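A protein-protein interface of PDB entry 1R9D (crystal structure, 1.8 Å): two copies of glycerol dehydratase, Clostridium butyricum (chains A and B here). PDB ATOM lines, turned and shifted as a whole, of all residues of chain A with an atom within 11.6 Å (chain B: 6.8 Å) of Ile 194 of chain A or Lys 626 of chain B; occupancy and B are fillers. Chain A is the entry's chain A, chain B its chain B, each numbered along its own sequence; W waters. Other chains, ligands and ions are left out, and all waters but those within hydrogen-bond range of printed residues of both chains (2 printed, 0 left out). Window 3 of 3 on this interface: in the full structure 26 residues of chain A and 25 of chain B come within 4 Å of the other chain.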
ATOM      1  N   LEU A 188      11.805 -28.391 -14.845  1.00  0.00           N
ATOM      2  CA  LEU A 188      12.322 -27.045 -14.662  1.00  0.00           C
ATOM      3  C   LEU A 188      13.653 -26.924 -15.416  1.00  0.00           C
ATOM      4  O   LEU A 188      13.943 -25.896 -16.035  1.00  0.00           O
ATOM      5  CB  LEU A 188      12.514 -26.790 -13.165  1.00  0.00           C
ATOM      6  CG  LEU A 188      12.085 -25.464 -12.532  1.00  0.00           C
ATOM      7  CD1 LEU A 188      10.798 -24.954 -13.150  1.00  0.00           C
ATOM      8  CD2 LEU A 188      11.910 -25.677 -11.030  1.00  0.00           C
ATOM      9  N   GLU A 189      14.455 -27.985 -15.374  1.00  0.00           N
ATOM     10  CA  GLU A 189      15.740 -27.987 -16.067  1.00  0.00           C
ATOM     11  C   GLU A 189      15.574 -28.099 -17.578  1.00  0.00           C
ATOM     12  O   GLU A 189      16.353 -27.522 -18.340  1.00  0.00           O
ATOM     13  CB  GLU A 189      16.624 -29.127 -15.559  1.00  0.00           C
ATOM     14  CG  GLU A 189      17.251 -28.842 -14.209  1.00  0.00           C
ATOM     15  CD  GLU A 189      18.004 -27.524 -14.200  1.00  0.00           C
ATOM     16  OE1 GLU A 189      18.979 -27.391 -14.972  1.00  0.00           O
ATOM     17  OE2 GLU A 189      17.617 -26.620 -13.427  1.00  0.00           O
ATOM     18  N   LYS A 190      14.564 -28.841 -18.012  1.00  0.00           N
ATOM     19  CA  LYS A 190      14.311 -28.999 -19.439  1.00  0.00           C
ATOM     20  C   LYS A 190      13.776 -27.692 -20.014  1.00  0.00           C
ATOM     21  O   LYS A 190      13.955 -27.404 -21.197  1.00  0.00           O
ATOM     22  CB  LYS A 190      13.289 -30.110 -19.687  1.00  0.00           C
ATOM     23  CG  LYS A 190      13.712 -31.485 -19.206  1.00  0.00           C
ATOM     24  CD  LYS A 190      12.623 -32.510 -19.489  1.00  0.00           C
ATOM     25  CE  LYS A 190      12.992 -33.886 -18.959  1.00  0.00           C
ATOM     26  NZ  LYS A 190      11.946 -34.904 -19.280  1.00  0.00           N
ATOM     27  N   ASN A 191      13.120 -26.907 -19.163  1.00  0.00           N
ATOM     28  CA  ASN A 191      12.530 -25.638 -19.568  1.00  0.00           C
ATOM     29  C   ASN A 191      13.469 -24.437 -19.566  1.00  0.00           C
ATOM     30  O   ASN A 191      13.091 -23.362 -20.034  1.00  0.00           O
ATOM     31  CB  ASN A 191      11.316 -25.320 -18.690  1.00  0.00           C
ATOM     32  CG  ASN A 191      10.125 -26.212 -18.995  1.00  0.00           C
ATOM     33  OD1 ASN A 191      10.192 -27.083 -19.860  1.00  0.00           O
ATOM     34  ND2 ASN A 191       9.027 -25.993 -18.281  1.00  0.00           N
ATOM     35  N   ARG A 192      14.678 -24.596 -19.037  1.00  0.00           N
ATOM     36  CA  ARG A 192      15.620 -23.479 -19.022  1.00  0.00           C
ATOM     37  C   ARG A 192      15.623 -22.891 -20.430  1.00  0.00           C
ATOM     38  O   ARG A 192      15.980 -23.570 -21.397  1.00  0.00           O
ATOM     39  CB  ARG A 192      17.025 -23.953 -18.633  1.00  0.00           C
ATOM     40  CG  ARG A 192      17.661 -24.938 -19.607  1.00  0.00           C
ATOM     41  CD  ARG A 192      19.100 -25.247 -19.209  1.00  0.00           C
ATOM     42  NE  ARG A 192      19.764 -26.121 -20.172  1.00  0.00           N
ATOM     43  CZ  ARG A 192      21.031 -26.511 -20.072  1.00  0.00           C
ATOM     44  NH1 ARG A 192      21.774 -26.103 -19.049  1.00  0.00           N
ATOM     45  NH2 ARG A 192      21.559 -27.309 -20.994  1.00  0.00           N
ATOM     46  N   SER A 193      15.208 -21.633 -20.545  1.00  0.00           N
ATOM     47  CA  SER A 193      15.132 -20.981 -21.848  1.00  0.00           C
ATOM     48  C   SER A 193      14.923 -19.477 -21.724  1.00  0.00           C
ATOM     49  O   SER A 193      14.508 -18.984 -20.676  1.00  0.00           O
ATOM     50  CB  SER A 193      13.973 -21.585 -22.649  1.00  0.00           C
ATOM     51  OG  SER A 193      13.684 -20.825 -23.810  1.00  0.00           O
ATOM     52  N   ILE A 194      15.210 -18.754 -22.802  1.00  0.00           N
ATOM     53  CA  ILE A 194      15.033 -17.307 -22.816  1.00  0.00           C
ATOM     54  C   ILE A 194      13.639 -16.938 -23.326  1.00  0.00           C
ATOM     55  O   ILE A 194      13.254 -15.768 -23.318  1.00  0.00           O
ATOM     56  CB  ILE A 194      16.099 -16.618 -23.697  1.00  0.00           C
ATOM     57  CG1 ILE A 194      16.075 -17.208 -25.109  1.00  0.00           C
ATOM     58  CG2 ILE A 194      17.482 -16.780 -23.062  1.00  0.00           C
ATOM     59  CD1 ILE A 194      16.943 -16.447 -26.101  1.00  0.00           C
ATOM     60  N   ASP A 195      12.888 -17.943 -23.764  1.00  0.00           N
ATOM     61  CA  ASP A 195      11.530 -17.738 -24.263  1.00  0.00           C
ATOM     62  C   ASP A 195      10.635 -17.282 -23.100  1.00  0.00           C
ATOM     63  O   ASP A 195      10.568 -17.945 -22.062  1.00  0.00           O
ATOM     64  CB  ASP A 195      10.985 -19.046 -24.844  1.00  0.00           C
ATOM     65  CG  ASP A 195       9.674 -18.858 -25.589  1.00  0.00           C
ATOM     66  OD1 ASP A 195       8.836 -18.043 -25.143  1.00  0.00           O
ATOM     67  OD2 ASP A 195       9.475 -19.541 -26.619  1.00  0.00           O
ATOM     68  N   PRO A 196       9.933 -16.148 -23.266  1.00  0.00           N
ATOM     69  CA  PRO A 196       9.036 -15.575 -22.253  1.00  0.00           C
ATOM     70  C   PRO A 196       7.953 -16.537 -21.766  1.00  0.00           C
ATOM     71  O   PRO A 196       7.507 -16.456 -20.618  1.00  0.00           O
ATOM     72  CB  PRO A 196       8.431 -14.367 -22.969  1.00  0.00           C
ATOM     73  CG  PRO A 196       9.468 -13.997 -23.960  1.00  0.00           C
ATOM     74  CD  PRO A 196       9.930 -15.321 -24.484  1.00  0.00           C
ATOM     75  N   ASP A 197       7.523 -17.443 -22.637  1.00  0.00           N
ATOM     76  CA  ASP A 197       6.483 -18.396 -22.264  1.00  0.00           C
ATOM     77  C   ASP A 197       6.859 -19.289 -21.088  1.00  0.00           C
ATOM     78  O   ASP A 197       5.990 -19.829 -20.411  1.00  0.00           O
ATOM     79  CB  ASP A 197       6.099 -19.275 -23.458  1.00  0.00           C
ATOM     80  CG  ASP A 197       5.252 -18.536 -24.478  1.00  0.00           C
ATOM     81  OD1 ASP A 197       4.334 -17.795 -24.059  1.00  0.00           O
ATOM     82  OD2 ASP A 197       5.491 -18.705 -25.696  1.00  0.00           O
ATOM     83  N   PHE A 198       8.150 -19.448 -20.830  1.00  0.00           N
ATOM     84  CA  PHE A 198       8.548 -20.305 -19.727  1.00  0.00           C
ATOM     85  C   PHE A 198       8.490 -19.621 -18.362  1.00  0.00           C
ATOM     86  O   PHE A 198       8.603 -20.285 -17.329  1.00  0.00           O
ATOM     87  CB  PHE A 198       9.937 -20.895 -19.987  1.00  0.00           C
ATOM     88  CG  PHE A 198       9.966 -21.894 -21.120  1.00  0.00           C
ATOM     89  CD1 PHE A 198      10.325 -21.505 -22.407  1.00  0.00           C
ATOM     90  CD2 PHE A 198       9.614 -23.223 -20.899  1.00  0.00           C
ATOM     91  CE1 PHE A 198      10.334 -22.424 -23.460  1.00  0.00           C
ATOM     92  CE2 PHE A 198       9.618 -24.151 -21.943  1.00  0.00           C
ATOM     93  CZ  PHE A 198       9.980 -23.750 -23.226  1.00  0.00           C
ATOM     94  N   ILE A 199       8.292 -18.306 -18.355  1.00  0.00           N
ATOM     95  CA  ILE A 199       8.209 -17.559 -17.098  1.00  0.00           C
ATOM     96  C   ILE A 199       7.028 -18.048 -16.255  1.00  0.00           C
ATOM     97  O   ILE A 199       7.187 -18.363 -15.074  1.00  0.00           O
ATOM     98  CB  ILE A 199       8.066 -16.037 -17.353  1.00  0.00           C
ATOM     99  CG1 ILE A 199       9.366 -15.488 -17.952  1.00  0.00           C
ATOM    100  CG2 ILE A 199       7.756 -15.309 -16.046  1.00  0.00           C
ATOM    101  CD1 ILE A 199       9.302 -14.029 -18.344  1.00  0.00           C
ATOM    102  N   LYS A 200       5.844 -18.126 -16.854  1.00  0.00           N
ATOM    103  CA  LYS A 200       4.682 -18.591 -16.105  1.00  0.00           C
ATOM    104  C   LYS A 200       4.766 -20.082 -15.791  1.00  0.00           C
ATOM    105  O   LYS A 200       4.302 -20.518 -14.741  1.00  0.00           O
ATOM    106  CB  LYS A 200       3.392 -18.282 -16.866  1.00  0.00           C
ATOM    107  CG  LYS A 200       3.030 -16.805 -16.855  1.00  0.00           C
ATOM    108  CD  LYS A 200       1.747 -16.536 -17.628  1.00  0.00           C
ATOM    109  CE  LYS A 200       1.439 -15.053 -17.677  1.00  0.00           C
ATOM    110  NZ  LYS A 200       0.198 -14.767 -18.454  1.00  0.00           N
ATOM    111  N   LYS A 201       5.361 -20.862 -16.688  1.00  0.00           N
ATOM    112  CA  LYS A 201       5.496 -22.297 -16.452  1.00  0.00           C
ATOM    113  C   LYS A 201       6.415 -22.512 -15.254  1.00  0.00           C
ATOM    114  O   LYS A 201       6.213 -23.424 -14.450  1.00  0.00           O
ATOM    115  CB  LYS A 201       6.083 -23.003 -17.677  1.00  0.00           C
ATOM    116  CG  LYS A 201       5.239 -22.893 -18.943  1.00  0.00           C
ATOM    117  CD  LYS A 201       5.836 -23.754 -20.055  1.00  0.00           C
ATOM    118  CE  LYS A 201       5.313 -23.362 -21.429  1.00  0.00           C
ATOM    119  NZ  LYS A 201       3.833 -23.411 -21.505  1.00  0.00           N
ATOM    120  N   GLU A 202       7.430 -21.661 -15.142  1.00  0.00           N
ATOM    121  CA  GLU A 202       8.382 -21.750 -14.047  1.00  0.00           C
ATOM    122  C   GLU A 202       7.659 -21.554 -12.715  1.00  0.00           C
ATOM    123  O   GLU A 202       7.881 -22.301 -11.760  1.00  0.00           O
ATOM    124  CB  GLU A 202       9.479 -20.697 -14.248  1.00  0.00           C
ATOM    125  CG  GLU A 202      10.590 -20.706 -13.220  1.00  0.00           C
ATOM    126  CD  GLU A 202      10.342 -19.727 -12.095  1.00  0.00           C
ATOM    127  OE1 GLU A 202       9.614 -20.080 -11.144  1.00  0.00           O
ATOM    128  OE2 GLU A 202      10.864 -18.593 -12.170  1.00  0.00           O
ATOM    129  N   LYS B 492      32.453 -10.434 -24.616  1.00  0.00           N
ATOM    130  CA  LYS B 492      31.194 -10.949 -25.146  1.00  0.00           C
ATOM    131  C   LYS B 492      30.469 -11.807 -24.112  1.00  0.00           C
ATOM    132  O   LYS B 492      29.239 -11.753 -24.003  1.00  0.00           O
ATOM    133  CB  LYS B 492      31.463 -11.755 -26.422  1.00  0.00           C
ATOM    134  CG  LYS B 492      30.228 -12.347 -27.102  1.00  0.00           C
ATOM    135  CD  LYS B 492      30.596 -12.859 -28.495  1.00  0.00           C
ATOM    136  CE  LYS B 492      29.446 -13.577 -29.184  1.00  0.00           C
ATOM    137  NZ  LYS B 492      29.136 -14.888 -28.550  1.00  0.00           N
ATOM    138  N   GLU B 496      26.814 -11.073 -22.707  1.00  0.00           N
ATOM    139  CA  GLU B 496      25.787 -12.102 -22.838  1.00  0.00           C
ATOM    140  C   GLU B 496      25.005 -12.346 -21.551  1.00  0.00           C
ATOM    141  O   GLU B 496      23.772 -12.404 -21.568  1.00  0.00           O
ATOM    142  CB  GLU B 496      26.431 -13.410 -23.312  1.00  0.00           C
ATOM    143  CG  GLU B 496      25.459 -14.533 -23.677  1.00  0.00           C
ATOM    144  CD  GLU B 496      24.810 -15.187 -22.470  1.00  0.00           C
ATOM    145  OE1 GLU B 496      25.526 -15.474 -21.486  1.00  0.00           O
ATOM    146  OE2 GLU B 496      23.583 -15.434 -22.509  1.00  0.00           O
ATOM    147  N   LYS B 500      21.063 -10.884 -21.040  1.00  0.00           N
ATOM    148  CA  LYS B 500      20.051 -11.919 -20.861  1.00  0.00           C
ATOM    149  C   LYS B 500      19.129 -11.568 -19.693  1.00  0.00           C
ATOM    150  O   LYS B 500      17.901 -11.602 -19.815  1.00  0.00           O
ATOM    151  CB  LYS B 500      20.710 -13.279 -20.591  1.00  0.00           C
ATOM    152  CG  LYS B 500      19.711 -14.420 -20.458  1.00  0.00           C
ATOM    153  CD  LYS B 500      20.196 -15.510 -19.512  1.00  0.00           C
ATOM    154  CE  LYS B 500      21.472 -16.169 -19.993  1.00  0.00           C
ATOM    155  NZ  LYS B 500      21.891 -17.252 -19.054  1.00  0.00           N
ATOM    156  N   CYS B 504      15.135 -10.483 -19.625  1.00  0.00           N
ATOM    157  CA  CYS B 504      14.216 -11.326 -18.867  1.00  0.00           C
ATOM    158  C   CYS B 504      13.471 -10.463 -17.850  1.00  0.00           C
ATOM    159  O   CYS B 504      12.272 -10.652 -17.628  1.00  0.00           O
ATOM    160  CB  CYS B 504      14.969 -12.463 -18.162  1.00  0.00           C
ATOM    161  SG  CYS B 504      15.599 -13.764 -19.294  1.00  0.00           S
ATOM    162  N   ASN B 507      10.801  -8.619 -19.618  1.00  0.00           N
ATOM    163  CA  ASN B 507       9.645  -9.464 -19.919  1.00  0.00           C
ATOM    164  C   ASN B 507       8.750  -9.704 -18.705  1.00  0.00           C
ATOM    165  O   ASN B 507       7.534  -9.844 -18.848  1.00  0.00           O
ATOM    166  CB  ASN B 507      10.092 -10.799 -20.530  1.00  0.00           C
ATOM    167  CG  ASN B 507      10.579 -10.643 -21.954  1.00  0.00           C
ATOM    168  OD1 ASN B 507      10.205  -9.693 -22.639  1.00  0.00           O
ATOM    169  ND2 ASN B 507      11.408 -11.581 -22.414  1.00  0.00           N
ATOM    170  N   CYS B 621      24.456  -4.950 -29.312  1.00  0.00           N
ATOM    171  CA  CYS B 621      23.320  -5.043 -30.223  1.00  0.00           C
ATOM    172  C   CYS B 621      22.965  -6.472 -30.629  1.00  0.00           C
ATOM    173  O   CYS B 621      21.782  -6.827 -30.711  1.00  0.00           O
ATOM    174  CB  CYS B 621      23.578  -4.186 -31.465  1.00  0.00           C
ATOM    175  SG  CYS B 621      23.658  -2.388 -31.118  1.00  0.00           S
ATOM    176  N   ARG B 622      23.978  -7.293 -30.883  1.00  0.00           N
ATOM    177  CA  ARG B 622      23.744  -8.680 -31.278  1.00  0.00           C
ATOM    178  C   ARG B 622      23.136  -9.500 -30.144  1.00  0.00           C
ATOM    179  O   ARG B 622      22.374 -10.437 -30.389  1.00  0.00           O
ATOM    180  CB  ARG B 622      25.043  -9.339 -31.735  1.00  0.00           C
ATOM    181  CG  ARG B 622      25.688  -8.695 -32.953  1.00  0.00           C
ATOM    182  CD  ARG B 622      26.898  -9.502 -33.394  1.00  0.00           C
ATOM    183  NE  ARG B 622      27.649  -8.855 -34.467  1.00  0.00           N
ATOM    184  CZ  ARG B 622      28.896  -8.411 -34.340  1.00  0.00           C
ATOM    185  NH1 ARG B 622      29.538  -8.544 -33.182  1.00  0.00           N
ATOM    186  NH2 ARG B 622      29.504  -7.838 -35.370  1.00  0.00           N
ATOM    187  N   GLU B 623      23.477  -9.166 -28.904  1.00  0.00           N
ATOM    188  CA  GLU B 623      22.916  -9.896 -27.778  1.00  0.00           C
ATOM    189  C   GLU B 623      21.438  -9.526 -27.639  1.00  0.00           C
ATOM    190  O   GLU B 623      20.585 -10.405 -27.504  1.00  0.00           O
ATOM    191  CB  GLU B 623      23.660  -9.568 -26.476  1.00  0.00           C
ATOM    192  CG  GLU B 623      25.059 -10.170 -26.363  1.00  0.00           C
ATOM    193  CD  GLU B 623      25.100 -11.669 -26.651  1.00  0.00           C
ATOM    194  OE1 GLU B 623      24.241 -12.419 -26.130  1.00  0.00           O
ATOM    195  OE2 GLU B 623      26.011 -12.104 -27.392  1.00  0.00           O
ATOM    196  N   VAL B 624      21.142  -8.229 -27.687  1.00  0.00           N
ATOM    197  CA  VAL B 624      19.763  -7.761 -27.565  1.00  0.00           C
ATOM    198  C   VAL B 624      18.835  -8.389 -28.613  1.00  0.00           C
ATOM    199  O   VAL B 624      17.710  -8.769 -28.296  1.00  0.00           O
ATOM    200  CB  VAL B 624      19.686  -6.219 -27.669  1.00  0.00           C
ATOM    201  CG1 VAL B 624      18.228  -5.761 -27.679  1.00  0.00           C
ATOM    202  CG2 VAL B 624      20.412  -5.585 -26.480  1.00  0.00           C
ATOM    203  N   ASN B 625      19.307  -8.504 -29.852  1.00  0.00           N
ATOM    204  CA  ASN B 625      18.504  -9.086 -30.935  1.00  0.00           C
ATOM    205  C   ASN B 625      18.050 -10.529 -30.706  1.00  0.00           C
ATOM    206  O   ASN B 625      17.140 -11.014 -31.386  1.00  0.00           O
ATOM    207  CB  ASN B 625      19.277  -9.031 -32.260  1.00  0.00           C
ATOM    208  CG  ASN B 625      19.145  -7.694 -32.969  1.00  0.00           C
ATOM    209  OD1 ASN B 625      18.413  -6.801 -32.530  1.00  0.00           O
ATOM    210  ND2 ASN B 625      19.856  -7.554 -34.087  1.00  0.00           N
ATOM    211  N   LYS B 626      18.668 -11.223 -29.758  1.00  0.00           N
ATOM    212  CA  LYS B 626      18.308 -12.618 -29.495  1.00  0.00           C
ATOM    213  C   LYS B 626      16.974 -12.812 -28.783  1.00  0.00           C
ATOM    214  O   LYS B 626      16.410 -13.912 -28.810  1.00  0.00           O
ATOM    215  CB  LYS B 626      19.384 -13.300 -28.645  1.00  0.00           C
ATOM    216  CG  LYS B 626      20.753 -13.434 -29.281  1.00  0.00           C
ATOM    217  CD  LYS B 626      21.739 -13.994 -28.264  1.00  0.00           C
ATOM    218  CE  LYS B 626      23.119 -14.216 -28.876  1.00  0.00           C
ATOM    219  NZ  LYS B 626      24.075 -14.755 -27.861  1.00  0.00           N
ATOM    220  N   TYR B 627      16.462 -11.752 -28.167  1.00  0.00           N
ATOM    221  CA  TYR B 627      15.236 -11.854 -27.374  1.00  0.00           C
ATOM    222  C   TYR B 627      13.895 -11.426 -27.959  1.00  0.00           C
ATOM    223  O   TYR B 627      13.828 -10.597 -28.867  1.00  0.00           O
ATOM    224  CB  TYR B 627      15.461 -11.125 -26.045  1.00  0.00           C
ATOM    225  CG  TYR B 627      16.682 -11.643 -25.334  1.00  0.00           C
ATOM    226  CD1 TYR B 627      17.957 -11.179 -25.662  1.00  0.00           C
ATOM    227  CD2 TYR B 627      16.578 -12.684 -24.414  1.00  0.00           C
ATOM    228  CE1 TYR B 627      19.099 -11.749 -25.099  1.00  0.00           C
ATOM    229  CE2 TYR B 627      17.710 -13.264 -23.848  1.00  0.00           C
ATOM    230  CZ  TYR B 627      18.967 -12.795 -24.200  1.00  0.00           C
ATOM    231  OH  TYR B 627      20.082 -13.416 -23.686  1.00  0.00           O
ATOM    232  N   THR B 628      12.831 -12.019 -27.418  1.00  0.00           N
ATOM    233  CA  THR B 628      11.464 -11.713 -27.824  1.00  0.00           C
ATOM    234  C   THR B 628      10.650 -11.397 -26.569  1.00  0.00           C
ATOM    235  O   THR B 628      11.003 -11.823 -25.467  1.00  0.00           O
ATOM    236  CB  THR B 628      10.800 -12.900 -28.560  1.00  0.00           C
ATOM    237  OG1 THR B 628      10.745 -14.033 -27.690  1.00  0.00           O
ATOM    238  CG2 THR B 628      11.589 -13.261 -29.810  1.00  0.00           C
ATOM    239  N   ASN B 634      10.034  -8.623 -31.235  1.00  0.00           N
ATOM    240  CA  ASN B 634      11.469  -8.747 -31.021  1.00  0.00           C
ATOM    241  C   ASN B 634      12.046  -7.546 -30.291  1.00  0.00           C
ATOM    242  O   ASN B 634      11.536  -6.426 -30.393  1.00  0.00           O
ATOM    243  CB  ASN B 634      12.221  -8.875 -32.351  1.00  0.00           C
ATOM    244  CG  ASN B 634      12.142 -10.262 -32.940  1.00  0.00           C
ATOM    245  OD1 ASN B 634      11.151 -10.629 -33.575  1.00  0.00           O
ATOM    246  ND2 ASN B 634      13.190 -11.051 -32.724  1.00  0.00           N
ATOM    247  N   PHE B 635      13.117  -7.794 -29.550  1.00  0.00           N
ATOM    248  CA  PHE B 635      13.817  -6.728 -28.850  1.00  0.00           C
ATOM    249  C   PHE B 635      14.692  -6.087 -29.925  1.00  0.00           C
ATOM    250  O   PHE B 635      15.161  -6.771 -30.842  1.00  0.00           O
ATOM    251  CB  PHE B 635      14.726  -7.296 -27.750  1.00  0.00           C
ATOM    252  CG  PHE B 635      14.049  -7.478 -26.423  1.00  0.00           C
ATOM    253  CD1 PHE B 635      13.031  -8.418 -26.261  1.00  0.00           C
ATOM    254  CD2 PHE B 635      14.451  -6.729 -25.318  1.00  0.00           C
ATOM    255  CE1 PHE B 635      12.426  -8.609 -25.020  1.00  0.00           C
ATOM    256  CE2 PHE B 635      13.851  -6.913 -24.069  1.00  0.00           C
ATOM    257  CZ  PHE B 635      12.837  -7.853 -23.920  1.00  0.00           C
HETATM  258  O   HOH W   1      13.453 -14.296 -25.601  1.00  0.00           O
HETATM  259  O   HOH W   2      12.229 -14.118 -21.042  1.00  0.00           O
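The backbone NH (N) of Phe 635 of chain B is in hydrogen-bond range of the backbone carbonyl oxygen (O) of Tyr 627 of chain B (3.0 Å).
The side-chain amide nitrogen of Asn 507 of chain B lies within hydrogen-bond range of the backbone carbonyl oxygen of Thr 628 of chain B, 3.1 Å away.
The side-chain carboxylate of Glu 623 of chain B is in salt-bridge range of the side-chain amino group of Lys 626 of chain B, at 2.9 Å.
Among the printed residues, merely in contact across the chains: Pro 196 of chain A with Thr 628 of chain B, Pro 196 of chain A with Asn 507 of chain B, Ile 194 of chain A with Tyr 627 of chain B, Ile 194 of chain A with Lys 626 of chain B and Ile 199 of chain A with Asn 507 of chain B.
Of the printed residues of chain B, Ile 194 of chain A touches Lys 626 and Tyr 627.
Asp 195 of chain A touches none of the printed residues of chain B.
Of the printed residues of chain B, Pro 196 of chain A touches Asn 507 (3.5 Å) and Thr 628 (3.1 Å).
Of the printed residues of chain B, Ile 199 of chain A touches Asn 507 (3.98 Å).
Glu 202 of chain A touches none of the printed residues of chain B.
No residue of chain A comes within 4 Å of Glu 496 of chain B.
Printed residues of chain A within 4 Å of Asn 507 of chain B: Pro 196 (3.5 Å) and Ile 199 (3.98 Å).
Glu 623 of chain B touches none of the printed residues of chain A.
Val 624 of chain B touches none of the printed residues of chain A.
No residue of chain A comes within 4 Å of Asn 625 of chain B.
Of the 15 printed residues of chain B, 4 touch a printed residue of chain A.
Along chain B the printed residues that touch a printed residue of chain A span positions 507 to 628.
Of the 15 printed residues of chain A, 3 touch a printed residue of chain B.
Among the printed residues, 5 pairs touch across the chains.
No position is printed for both chains.
Of the 5 pairs that touch across the chains among the printed residues, none has its exchanged pair printed and touching as well.
Water W1 lies within hydrogen-bond range of O of Ile 194 of chain A and N of Thr 628 of chain B.
Water W2 bridges the backbone carbonyl oxygen of Ile 194 of chain A and the side-chain amide nitrogen of Asn 507 of chain B.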
